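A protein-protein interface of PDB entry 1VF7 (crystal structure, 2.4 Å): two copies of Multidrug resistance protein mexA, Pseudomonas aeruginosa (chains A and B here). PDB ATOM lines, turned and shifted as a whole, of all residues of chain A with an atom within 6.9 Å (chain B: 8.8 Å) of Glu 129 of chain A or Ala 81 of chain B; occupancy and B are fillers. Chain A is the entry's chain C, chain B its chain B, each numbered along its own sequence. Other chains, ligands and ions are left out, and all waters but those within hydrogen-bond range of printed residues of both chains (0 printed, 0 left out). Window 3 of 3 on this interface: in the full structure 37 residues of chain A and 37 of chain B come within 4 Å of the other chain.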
ATOM      1  N   TYR A  83      -6.896   6.612  -6.721  1.00  0.00           N
ATOM      2  CA  TYR A  83      -6.138   7.626  -6.079  1.00  0.00           C
ATOM      3  C   TYR A  83      -6.050   7.394  -4.559  1.00  0.00           C
ATOM      4  O   TYR A  83      -4.942   7.415  -3.995  1.00  0.00           O
ATOM      5  CB  TYR A  83      -6.767   9.008  -6.416  1.00  0.00           C
ATOM      6  CG  TYR A  83      -6.086  10.143  -5.739  1.00  0.00           C
ATOM      7  CD1 TYR A  83      -4.718  10.412  -5.957  1.00  0.00           C
ATOM      8  CD2 TYR A  83      -6.785  10.972  -4.922  1.00  0.00           C
ATOM      9  CE1 TYR A  83      -4.092  11.445  -5.389  1.00  0.00           C
ATOM     10  CE2 TYR A  83      -6.185  12.055  -4.323  1.00  0.00           C
ATOM     11  CZ  TYR A  83      -4.837  12.284  -4.562  1.00  0.00           C
ATOM     12  OH  TYR A  83      -4.279  13.367  -3.949  1.00  0.00           O
ATOM     13  N   ALA A  86      -3.776   4.445  -3.845  1.00  0.00           N
ATOM     14  CA  ALA A  86      -2.401   4.843  -4.044  1.00  0.00           C
ATOM     15  C   ALA A  86      -1.952   5.725  -2.867  1.00  0.00           C
ATOM     16  O   ALA A  86      -0.848   5.551  -2.316  1.00  0.00           O
ATOM     17  CB  ALA A  86      -2.213   5.577  -5.435  1.00  0.00           C
ATOM     18  N   SER A 124       5.358   3.960  -5.128  1.00  0.00           N
ATOM     19  CA  SER A 124       4.154   4.590  -4.578  1.00  0.00           C
ATOM     20  C   SER A 124       4.054   6.055  -4.892  1.00  0.00           C
ATOM     21  O   SER A 124       2.956   6.527  -5.168  1.00  0.00           O
ATOM     22  CB  SER A 124       3.971   4.417  -3.030  1.00  0.00           C
ATOM     23  OG  SER A 124       4.163   3.072  -2.674  1.00  0.00           O
ATOM     24  N   LYS A 125       5.161   6.788  -4.819  1.00  0.00           N
ATOM     25  CA  LYS A 125       5.185   8.200  -5.212  1.00  0.00           C
ATOM     26  C   LYS A 125       4.727   8.372  -6.647  1.00  0.00           C
ATOM     27  O   LYS A 125       3.847   9.138  -6.925  1.00  0.00           O
ATOM     28  CB  LYS A 125       6.568   8.833  -5.014  1.00  0.00           C
ATOM     29  CG  LYS A 125       6.587   9.748  -3.823  1.00  0.00           C
ATOM     30  CD  LYS A 125       7.810  10.691  -3.829  1.00  0.00           C
ATOM     31  CE  LYS A 125       7.553  11.992  -4.643  1.00  0.00           C
ATOM     32  NZ  LYS A 125       8.603  13.091  -4.414  1.00  0.00           N
ATOM     33  N   ALA A 126       5.261   7.577  -7.543  1.00  0.00           N
ATOM     34  CA  ALA A 126       4.941   7.703  -8.938  1.00  0.00           C
ATOM     35  C   ALA A 126       3.464   7.371  -9.154  1.00  0.00           C
ATOM     36  O   ALA A 126       2.727   8.144  -9.774  1.00  0.00           O
ATOM     37  CB  ALA A 126       5.884   6.766  -9.788  1.00  0.00           C
ATOM     38  N   ALA A 127       2.987   6.280  -8.559  1.00  0.00           N
ATOM     39  CA  ALA A 127       1.566   5.865  -8.668  1.00  0.00           C
ATOM     40  C   ALA A 127       0.578   6.893  -8.106  1.00  0.00           C
ATOM     41  O   ALA A 127      -0.447   7.175  -8.736  1.00  0.00           O
ATOM     42  CB  ALA A 127       1.373   4.455  -8.068  1.00  0.00           C
ATOM     43  N   VAL A 128       0.933   7.564  -7.012  1.00  0.00           N
ATOM     44  CA  VAL A 128       0.091   8.667  -6.512  1.00  0.00           C
ATOM     45  C   VAL A 128      -0.011   9.829  -7.477  1.00  0.00           C
ATOM     46  O   VAL A 128      -1.138  10.387  -7.726  1.00  0.00           O
ATOM     47  CB  VAL A 128       0.534   9.157  -5.118  1.00  0.00           C
ATOM     48  CG1 VAL A 128      -0.210  10.417  -4.681  1.00  0.00           C
ATOM     49  CG2 VAL A 128       0.293   8.059  -4.154  1.00  0.00           C
ATOM     50  N   GLU A 129       1.111  10.170  -8.107  1.00  0.00           N
ATOM     51  CA  GLU A 129       1.135  11.388  -8.925  1.00  0.00           C
ATOM     52  C   GLU A 129       0.311  11.169 -10.175  1.00  0.00           C
ATOM     53  O   GLU A 129      -0.471  12.007 -10.573  1.00  0.00           O
ATOM     54  CB  GLU A 129       2.597  11.778  -9.217  1.00  0.00           C
ATOM     55  CG  GLU A 129       2.704  13.040 -10.069  1.00  0.00           C
ATOM     56  CD  GLU A 129       1.892  14.246  -9.539  1.00  0.00           C
ATOM     57  OE1 GLU A 129       1.664  14.394  -8.275  1.00  0.00           O
ATOM     58  OE2 GLU A 129       1.493  15.047 -10.422  1.00  0.00           O
ATOM     59  N   GLN A 130       0.442   9.996 -10.754  1.00  0.00           N
ATOM     60  CA  GLN A 130      -0.355   9.628 -11.899  1.00  0.00           C
ATOM     61  C   GLN A 130      -1.831   9.500 -11.609  1.00  0.00           C
ATOM     62  O   GLN A 130      -2.652   9.888 -12.452  1.00  0.00           O
ATOM     63  CB  GLN A 130       0.134   8.311 -12.481  1.00  0.00           C
ATOM     64  CG  GLN A 130      -0.458   8.063 -13.910  1.00  0.00           C
ATOM     65  CD  GLN A 130      -0.225   9.297 -14.876  1.00  0.00           C
ATOM     66  OE1 GLN A 130       0.944   9.748 -15.062  1.00  0.00           O
ATOM     67  NE2 GLN A 130      -1.340   9.859 -15.439  1.00  0.00           N
ATOM     68  N   ALA A 131      -2.220   8.929 -10.441  1.00  0.00           N
ATOM     69  CA  ALA A 131      -3.645   8.770 -10.123  1.00  0.00           C
ATOM     70  C   ALA A 131      -4.215  10.160  -9.857  1.00  0.00           C
ATOM     71  O   ALA A 131      -5.397  10.461 -10.158  1.00  0.00           O
ATOM     72  CB  ALA A 131      -3.821   7.846  -8.875  1.00  0.00           C
ATOM     73  N   ARG A 132      -3.384  11.060  -9.348  1.00  0.00           N
ATOM     74  CA  ARG A 132      -3.854  12.446  -9.093  1.00  0.00           C
ATOM     75  C   ARG A 132      -4.144  13.143 -10.420  1.00  0.00           C
ATOM     76  O   ARG A 132      -5.189  13.794 -10.591  1.00  0.00           O
ATOM     77  CB  ARG A 132      -2.823  13.210  -8.288  1.00  0.00           C
ATOM     78  CG  ARG A 132      -3.242  14.663  -7.894  1.00  0.00           C
ATOM     79  CD  ARG A 132      -2.094  15.480  -7.326  1.00  0.00           C
ATOM     80  NE  ARG A 132      -1.102  15.832  -8.431  1.00  0.00           N
ATOM     81  CZ  ARG A 132      -1.306  16.528  -9.627  1.00  0.00           C
ATOM     82  NH1 ARG A 132      -2.514  16.959 -10.092  1.00  0.00           N
ATOM     83  NH2 ARG A 132      -0.248  16.737 -10.394  1.00  0.00           N
ATOM     84  N   ILE A 133      -3.284  12.945 -11.419  1.00  0.00           N
ATOM     85  CA  ILE A 133      -3.471  13.642 -12.680  1.00  0.00           C
ATOM     86  C   ILE A 133      -4.726  13.111 -13.389  1.00  0.00           C
ATOM     87  O   ILE A 133      -5.562  13.902 -13.862  1.00  0.00           O
ATOM     88  CB  ILE A 133      -2.171  13.489 -13.563  1.00  0.00           C
ATOM     89  CG1 ILE A 133      -0.989  14.314 -12.976  1.00  0.00           C
ATOM     90  CG2 ILE A 133      -2.431  13.919 -15.066  1.00  0.00           C
ATOM     91  CD1 ILE A 133       0.413  13.832 -13.613  1.00  0.00           C
ATOM     92  N   ASN A 134      -4.885  11.788 -13.460  1.00  0.00           N
ATOM     93  CA  ASN A 134      -6.066  11.181 -14.104  1.00  0.00           C
ATOM     94  C   ASN A 134      -7.329  11.650 -13.515  1.00  0.00           C
ATOM     95  O   ASN A 134      -8.280  11.988 -14.250  1.00  0.00           O
ATOM     96  CB  ASN A 134      -6.022   9.693 -13.995  1.00  0.00           C
ATOM     97  CG  ASN A 134      -4.859   9.085 -14.827  1.00  0.00           C
ATOM     98  OD1 ASN A 134      -4.248   9.766 -15.665  1.00  0.00           O
ATOM     99  ND2 ASN A 134      -4.561   7.798 -14.595  1.00  0.00           N
ATOM    100  N   ARG A 136      -7.714  14.456 -11.791  1.00  0.00           N
ATOM    101  CA  ARG A 136      -7.962  15.889 -12.093  1.00  0.00           C
ATOM    102  C   ARG A 136      -8.660  15.999 -13.469  1.00  0.00           C
ATOM    103  O   ARG A 136      -9.586  16.748 -13.612  1.00  0.00           O
ATOM    104  CB  ARG A 136      -6.629  16.638 -12.132  1.00  0.00           C
ATOM    105  CG  ARG A 136      -6.712  18.147 -12.397  1.00  0.00           C
ATOM    106  CD  ARG A 136      -5.250  18.892 -12.389  1.00  0.00           C
ATOM    107  NE  ARG A 136      -4.992  19.308 -13.788  1.00  0.00           N
ATOM    108  CZ  ARG A 136      -3.918  19.020 -14.515  1.00  0.00           C
ATOM    109  NH1 ARG A 136      -2.870  18.333 -14.038  1.00  0.00           N
ATOM    110  NH2 ARG A 136      -3.913  19.466 -15.747  1.00  0.00           N
ATOM    111  N   PRO B  76       2.022  19.559 -20.218  1.00  0.00           N
ATOM    112  CA  PRO B  76       3.106  18.735 -19.825  1.00  0.00           C
ATOM    113  C   PRO B  76       2.857  17.879 -18.556  1.00  0.00           C
ATOM    114  O   PRO B  76       3.787  17.188 -18.123  1.00  0.00           O
ATOM    115  CB  PRO B  76       4.165  19.810 -19.409  1.00  0.00           C
ATOM    116  CG  PRO B  76       3.385  20.795 -18.692  1.00  0.00           C
ATOM    117  CD  PRO B  76       2.078  20.884 -19.522  1.00  0.00           C
ATOM    118  N   ALA B  77       1.673  17.937 -17.930  1.00  0.00           N
ATOM    119  CA  ALA B  77       1.459  17.147 -16.634  1.00  0.00           C
ATOM    120  C   ALA B  77       2.039  15.705 -16.590  1.00  0.00           C
ATOM    121  O   ALA B  77       2.856  15.349 -15.734  1.00  0.00           O
ATOM    122  CB  ALA B  77       0.047  17.141 -16.278  1.00  0.00           C
ATOM    123  N   THR B  78       1.611  14.859 -17.498  1.00  0.00           N
ATOM    124  CA  THR B  78       2.069  13.453 -17.524  1.00  0.00           C
ATOM    125  C   THR B  78       3.536  13.258 -17.949  1.00  0.00           C
ATOM    126  O   THR B  78       4.224  12.349 -17.430  1.00  0.00           O
ATOM    127  CB  THR B  78       1.222  12.740 -18.560  1.00  0.00           C
ATOM    128  OG1 THR B  78      -0.140  12.845 -18.189  1.00  0.00           O
ATOM    129  CG2 THR B  78       1.491  11.260 -18.589  1.00  0.00           C
ATOM    130  N   TYR B  79       3.974  14.015 -18.975  1.00  0.00           N
ATOM    131  CA  TYR B  79       5.400  14.091 -19.365  1.00  0.00           C
ATOM    132  C   TYR B  79       6.229  14.480 -18.189  1.00  0.00           C
ATOM    133  O   TYR B  79       7.291  13.942 -17.976  1.00  0.00           O
ATOM    134  CB  TYR B  79       5.676  15.091 -20.556  1.00  0.00           C
ATOM    135  CG  TYR B  79       5.152  14.586 -21.851  1.00  0.00           C
ATOM    136  CD1 TYR B  79       4.121  15.239 -22.483  1.00  0.00           C
ATOM    137  CD2 TYR B  79       5.633  13.390 -22.407  1.00  0.00           C
ATOM    138  CE1 TYR B  79       3.535  14.741 -23.672  1.00  0.00           C
ATOM    139  CE2 TYR B  79       5.094  12.864 -23.614  1.00  0.00           C
ATOM    140  CZ  TYR B  79       4.019  13.587 -24.240  1.00  0.00           C
ATOM    141  OH  TYR B  79       3.432  13.158 -25.435  1.00  0.00           O
ATOM    142  N   GLU B  80       5.761  15.410 -17.410  1.00  0.00           N
ATOM    143  CA  GLU B  80       6.534  15.800 -16.248  1.00  0.00           C
ATOM    144  C   GLU B  80       6.584  14.637 -15.191  1.00  0.00           C
ATOM    145  O   GLU B  80       7.620  14.380 -14.630  1.00  0.00           O
ATOM    146  CB  GLU B  80       5.965  17.066 -15.682  1.00  0.00           C
ATOM    147  CG  GLU B  80       6.561  17.424 -14.343  1.00  0.00           C
ATOM    148  CD  GLU B  80       7.960  18.026 -14.498  1.00  0.00           C
ATOM    149  OE1 GLU B  80       8.020  19.124 -15.130  1.00  0.00           O
ATOM    150  OE2 GLU B  80       8.985  17.414 -14.036  1.00  0.00           O
ATOM    151  N   ALA B  81       5.482  13.920 -15.007  1.00  0.00           N
ATOM    152  CA  ALA B  81       5.378  12.810 -14.010  1.00  0.00           C
ATOM    153  C   ALA B  81       6.187  11.627 -14.483  1.00  0.00           C
ATOM    154  O   ALA B  81       6.926  11.089 -13.697  1.00  0.00           O
ATOM    155  CB  ALA B  81       3.863  12.356 -13.775  1.00  0.00           C
ATOM    156  N   ASP B  82       6.096  11.269 -15.771  1.00  0.00           N
ATOM    157  CA  ASP B  82       6.984  10.237 -16.354  1.00  0.00           C
ATOM    158  C   ASP B  82       8.457  10.507 -16.199  1.00  0.00           C
ATOM    159  O   ASP B  82       9.247   9.622 -15.897  1.00  0.00           O
ATOM    160  CB  ASP B  82       6.664   9.999 -17.827  1.00  0.00           C
ATOM    161  CG  ASP B  82       5.300   9.358 -18.003  1.00  0.00           C
ATOM    162  OD1 ASP B  82       4.683   8.990 -16.967  1.00  0.00           O
ATOM    163  OD2 ASP B  82       4.720   9.205 -19.098  1.00  0.00           O
ATOM    164  N   TYR B  83       8.846  11.751 -16.350  1.00  0.00           N
ATOM    165  CA  TYR B  83      10.252  12.082 -16.214  1.00  0.00           C
ATOM    166  C   TYR B  83      10.713  11.963 -14.757  1.00  0.00           C
ATOM    167  O   TYR B  83      11.726  11.356 -14.478  1.00  0.00           O
ATOM    168  CB  TYR B  83      10.481  13.506 -16.775  1.00  0.00           C
ATOM    169  CG  TYR B  83      11.879  13.995 -16.615  1.00  0.00           C
ATOM    170  CD1 TYR B  83      12.968  13.292 -17.203  1.00  0.00           C
ATOM    171  CD2 TYR B  83      12.136  15.130 -15.893  1.00  0.00           C
ATOM    172  CE1 TYR B  83      14.259  13.717 -17.084  1.00  0.00           C
ATOM    173  CE2 TYR B  83      13.442  15.584 -15.759  1.00  0.00           C
ATOM    174  CZ  TYR B  83      14.480  14.854 -16.357  1.00  0.00           C
ATOM    175  OH  TYR B  83      15.758  15.315 -16.219  1.00  0.00           O
ATOM    176  N   GLN B  84       9.964  12.541 -13.838  1.00  0.00           N
ATOM    177  CA  GLN B  84      10.178  12.383 -12.380  1.00  0.00           C
ATOM    178  C   GLN B  84      10.251  10.913 -11.919  1.00  0.00           C
ATOM    179  O   GLN B  84      11.131  10.460 -11.194  1.00  0.00           O
ATOM    180  CB  GLN B  84       9.009  13.027 -11.675  1.00  0.00           C
ATOM    181  CG  GLN B  84       9.454  14.015 -10.697  1.00  0.00           C
ATOM    182  CD  GLN B  84       9.688  15.387 -11.315  1.00  0.00           C
ATOM    183  OE1 GLN B  84       8.711  16.184 -11.467  1.00  0.00           O
ATOM    184  NE2 GLN B  84      10.965  15.697 -11.659  1.00  0.00           N
ATOM    185  N   SER B  85       9.294  10.175 -12.378  1.00  0.00           N
ATOM    186  CA  SER B  85       9.200   8.768 -12.139  1.00  0.00           C
ATOM    187  C   SER B  85      10.421   7.947 -12.734  1.00  0.00           C
ATOM    188  O   SER B  85      10.991   7.041 -12.067  1.00  0.00           O
ATOM    189  CB  SER B  85       7.911   8.363 -12.807  1.00  0.00           C
ATOM    190  OG  SER B  85       7.768   7.016 -12.701  1.00  0.00           O
ATOM    191  N   ALA B  86      10.817   8.255 -13.971  1.00  0.00           N
ATOM    192  CA  ALA B  86      12.027   7.654 -14.581  1.00  0.00           C
ATOM    193  C   ALA B  86      13.280   8.042 -13.839  1.00  0.00           C
ATOM    194  O   ALA B  86      14.199   7.240 -13.704  1.00  0.00           O
ATOM    195  CB  ALA B  86      12.165   8.073 -16.074  1.00  0.00           C
ATOM    196  N   GLN B  87      13.340   9.274 -13.346  1.00  0.00           N
ATOM    197  CA  GLN B  87      14.477   9.684 -12.527  1.00  0.00           C
ATOM    198  C   GLN B  87      14.606   8.907 -11.233  1.00  0.00           C
ATOM    199  O   GLN B  87      15.743   8.614 -10.784  1.00  0.00           O
ATOM    200  CB  GLN B  87      14.370  11.167 -12.181  1.00  0.00           C
ATOM    201  CG  GLN B  87      14.768  11.985 -13.362  1.00  0.00           C
ATOM    202  CD  GLN B  87      14.981  13.438 -13.061  1.00  0.00           C
ATOM    203  OE1 GLN B  87      14.060  14.167 -12.625  1.00  0.00           O
ATOM    204  NE2 GLN B  87      16.202  13.894 -13.338  1.00  0.00           N
ATOM    205  N   ALA B  88      13.453   8.587 -10.622  1.00  0.00           N
ATOM    206  CA  ALA B  88      13.442   7.892  -9.343  1.00  0.00           C
ATOM    207  C   ALA B  88      13.798   6.412  -9.538  1.00  0.00           C
ATOM    208  O   ALA B  88      14.486   5.880  -8.699  1.00  0.00           O
ATOM    209  CB  ALA B  88      12.058   8.055  -8.588  1.00  0.00           C
ATOM    210  N   ALA B 131      12.450  10.353 -21.612  1.00  0.00           N
ATOM    211  CA  ALA B 131      11.481  11.159 -20.931  1.00  0.00           C
ATOM    212  C   ALA B 131      11.933  12.635 -20.915  1.00  0.00           C
ATOM    213  O   ALA B 131      11.105  13.528 -21.050  1.00  0.00           O
ATOM    214  CB  ALA B 131      11.211  10.643 -19.512  1.00  0.00           C
ATOM    215  N   LEU B 135       9.773  15.755 -22.628  1.00  0.00           N
ATOM    216  CA  LEU B 135       9.336  16.822 -21.790  1.00  0.00           C
ATOM    217  C   LEU B 135       9.864  18.171 -22.365  1.00  0.00           C
ATOM    218  O   LEU B 135       9.179  19.199 -22.338  1.00  0.00           O
ATOM    219  CB  LEU B 135       9.789  16.568 -20.339  1.00  0.00           C
ATOM    220  CG  LEU B 135       9.581  17.765 -19.354  1.00  0.00           C
ATOM    221  CD1 LEU B 135       8.095  18.230 -19.155  1.00  0.00           C
ATOM    222  CD2 LEU B 135      10.289  17.554 -17.980  1.00  0.00           C
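The side-chain carboxylate (OE2) of Glu 129 of chain A is in salt-bridge range of the guanidinium group (NH2) of Arg 132 of chain A (2.4 Å).
NE2 of Gln 130 of chain A lies within hydrogen-bond range of OD1 of Asn 134 of chain A, 2.9 Å away.
Among the printed residues, merely in contact across the chains: Ala 126 of chain A with Ser 85 of chain B, Ile 133 of chain A with Ala 77 of chain B, Ile 133 of chain A with Ala 81 of chain B, Arg 136 of chain A with Ala 77 of chain B, Gln 130 of chain A with Thr 78 of chain B and Glu 129 of chain A with Ala 81 of chain B.
No residue of chain B comes within 4 Å of Val 128 of chain A.
Of the printed residues of chain B, Ile 133 of chain A touches Ala 77 and Ala 81.
Printed residues of chain B within 4 Å of Arg 136 of chain A: Ala 77 (3.9 Å).
Ala 81 of chain B touches two residues of chain A.
Printed residues of chain A within 4 Å of Ser 85 of chain B: Ala 126 (3.5 Å).
The nearest residue of chain B that does not touch Glu 129 of chain A is Ala 77 of chain B (5.5 Å).
Of the 14 printed residues of chain A, 5 touch a printed residue of chain B.
Hydrophobic or aromatic side chains of chain A that line the printed part of chain B: Ala 126 and Ile 133.
Printed residues of chain B that touch a printed residue of chain A: Ala 77, Thr 78, Ala 81 and Ser 85.
Hydrophobic or aromatic side chains of chain B that line the printed part of chain A: Ala 77 and Ala 81.
Among the printed residues, 6 pairs touch across the chains.
Among the printed residues, no Asp or Glu carboxylate lies within 4 Å of a Lys or Arg side-chain nitrogen of the other chain.
Positions printed for both chains: 83, 86 and 131.
Of the 6 pairs that touch across the chains among the printed residues, none has its exchanged pair printed and touching as well.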
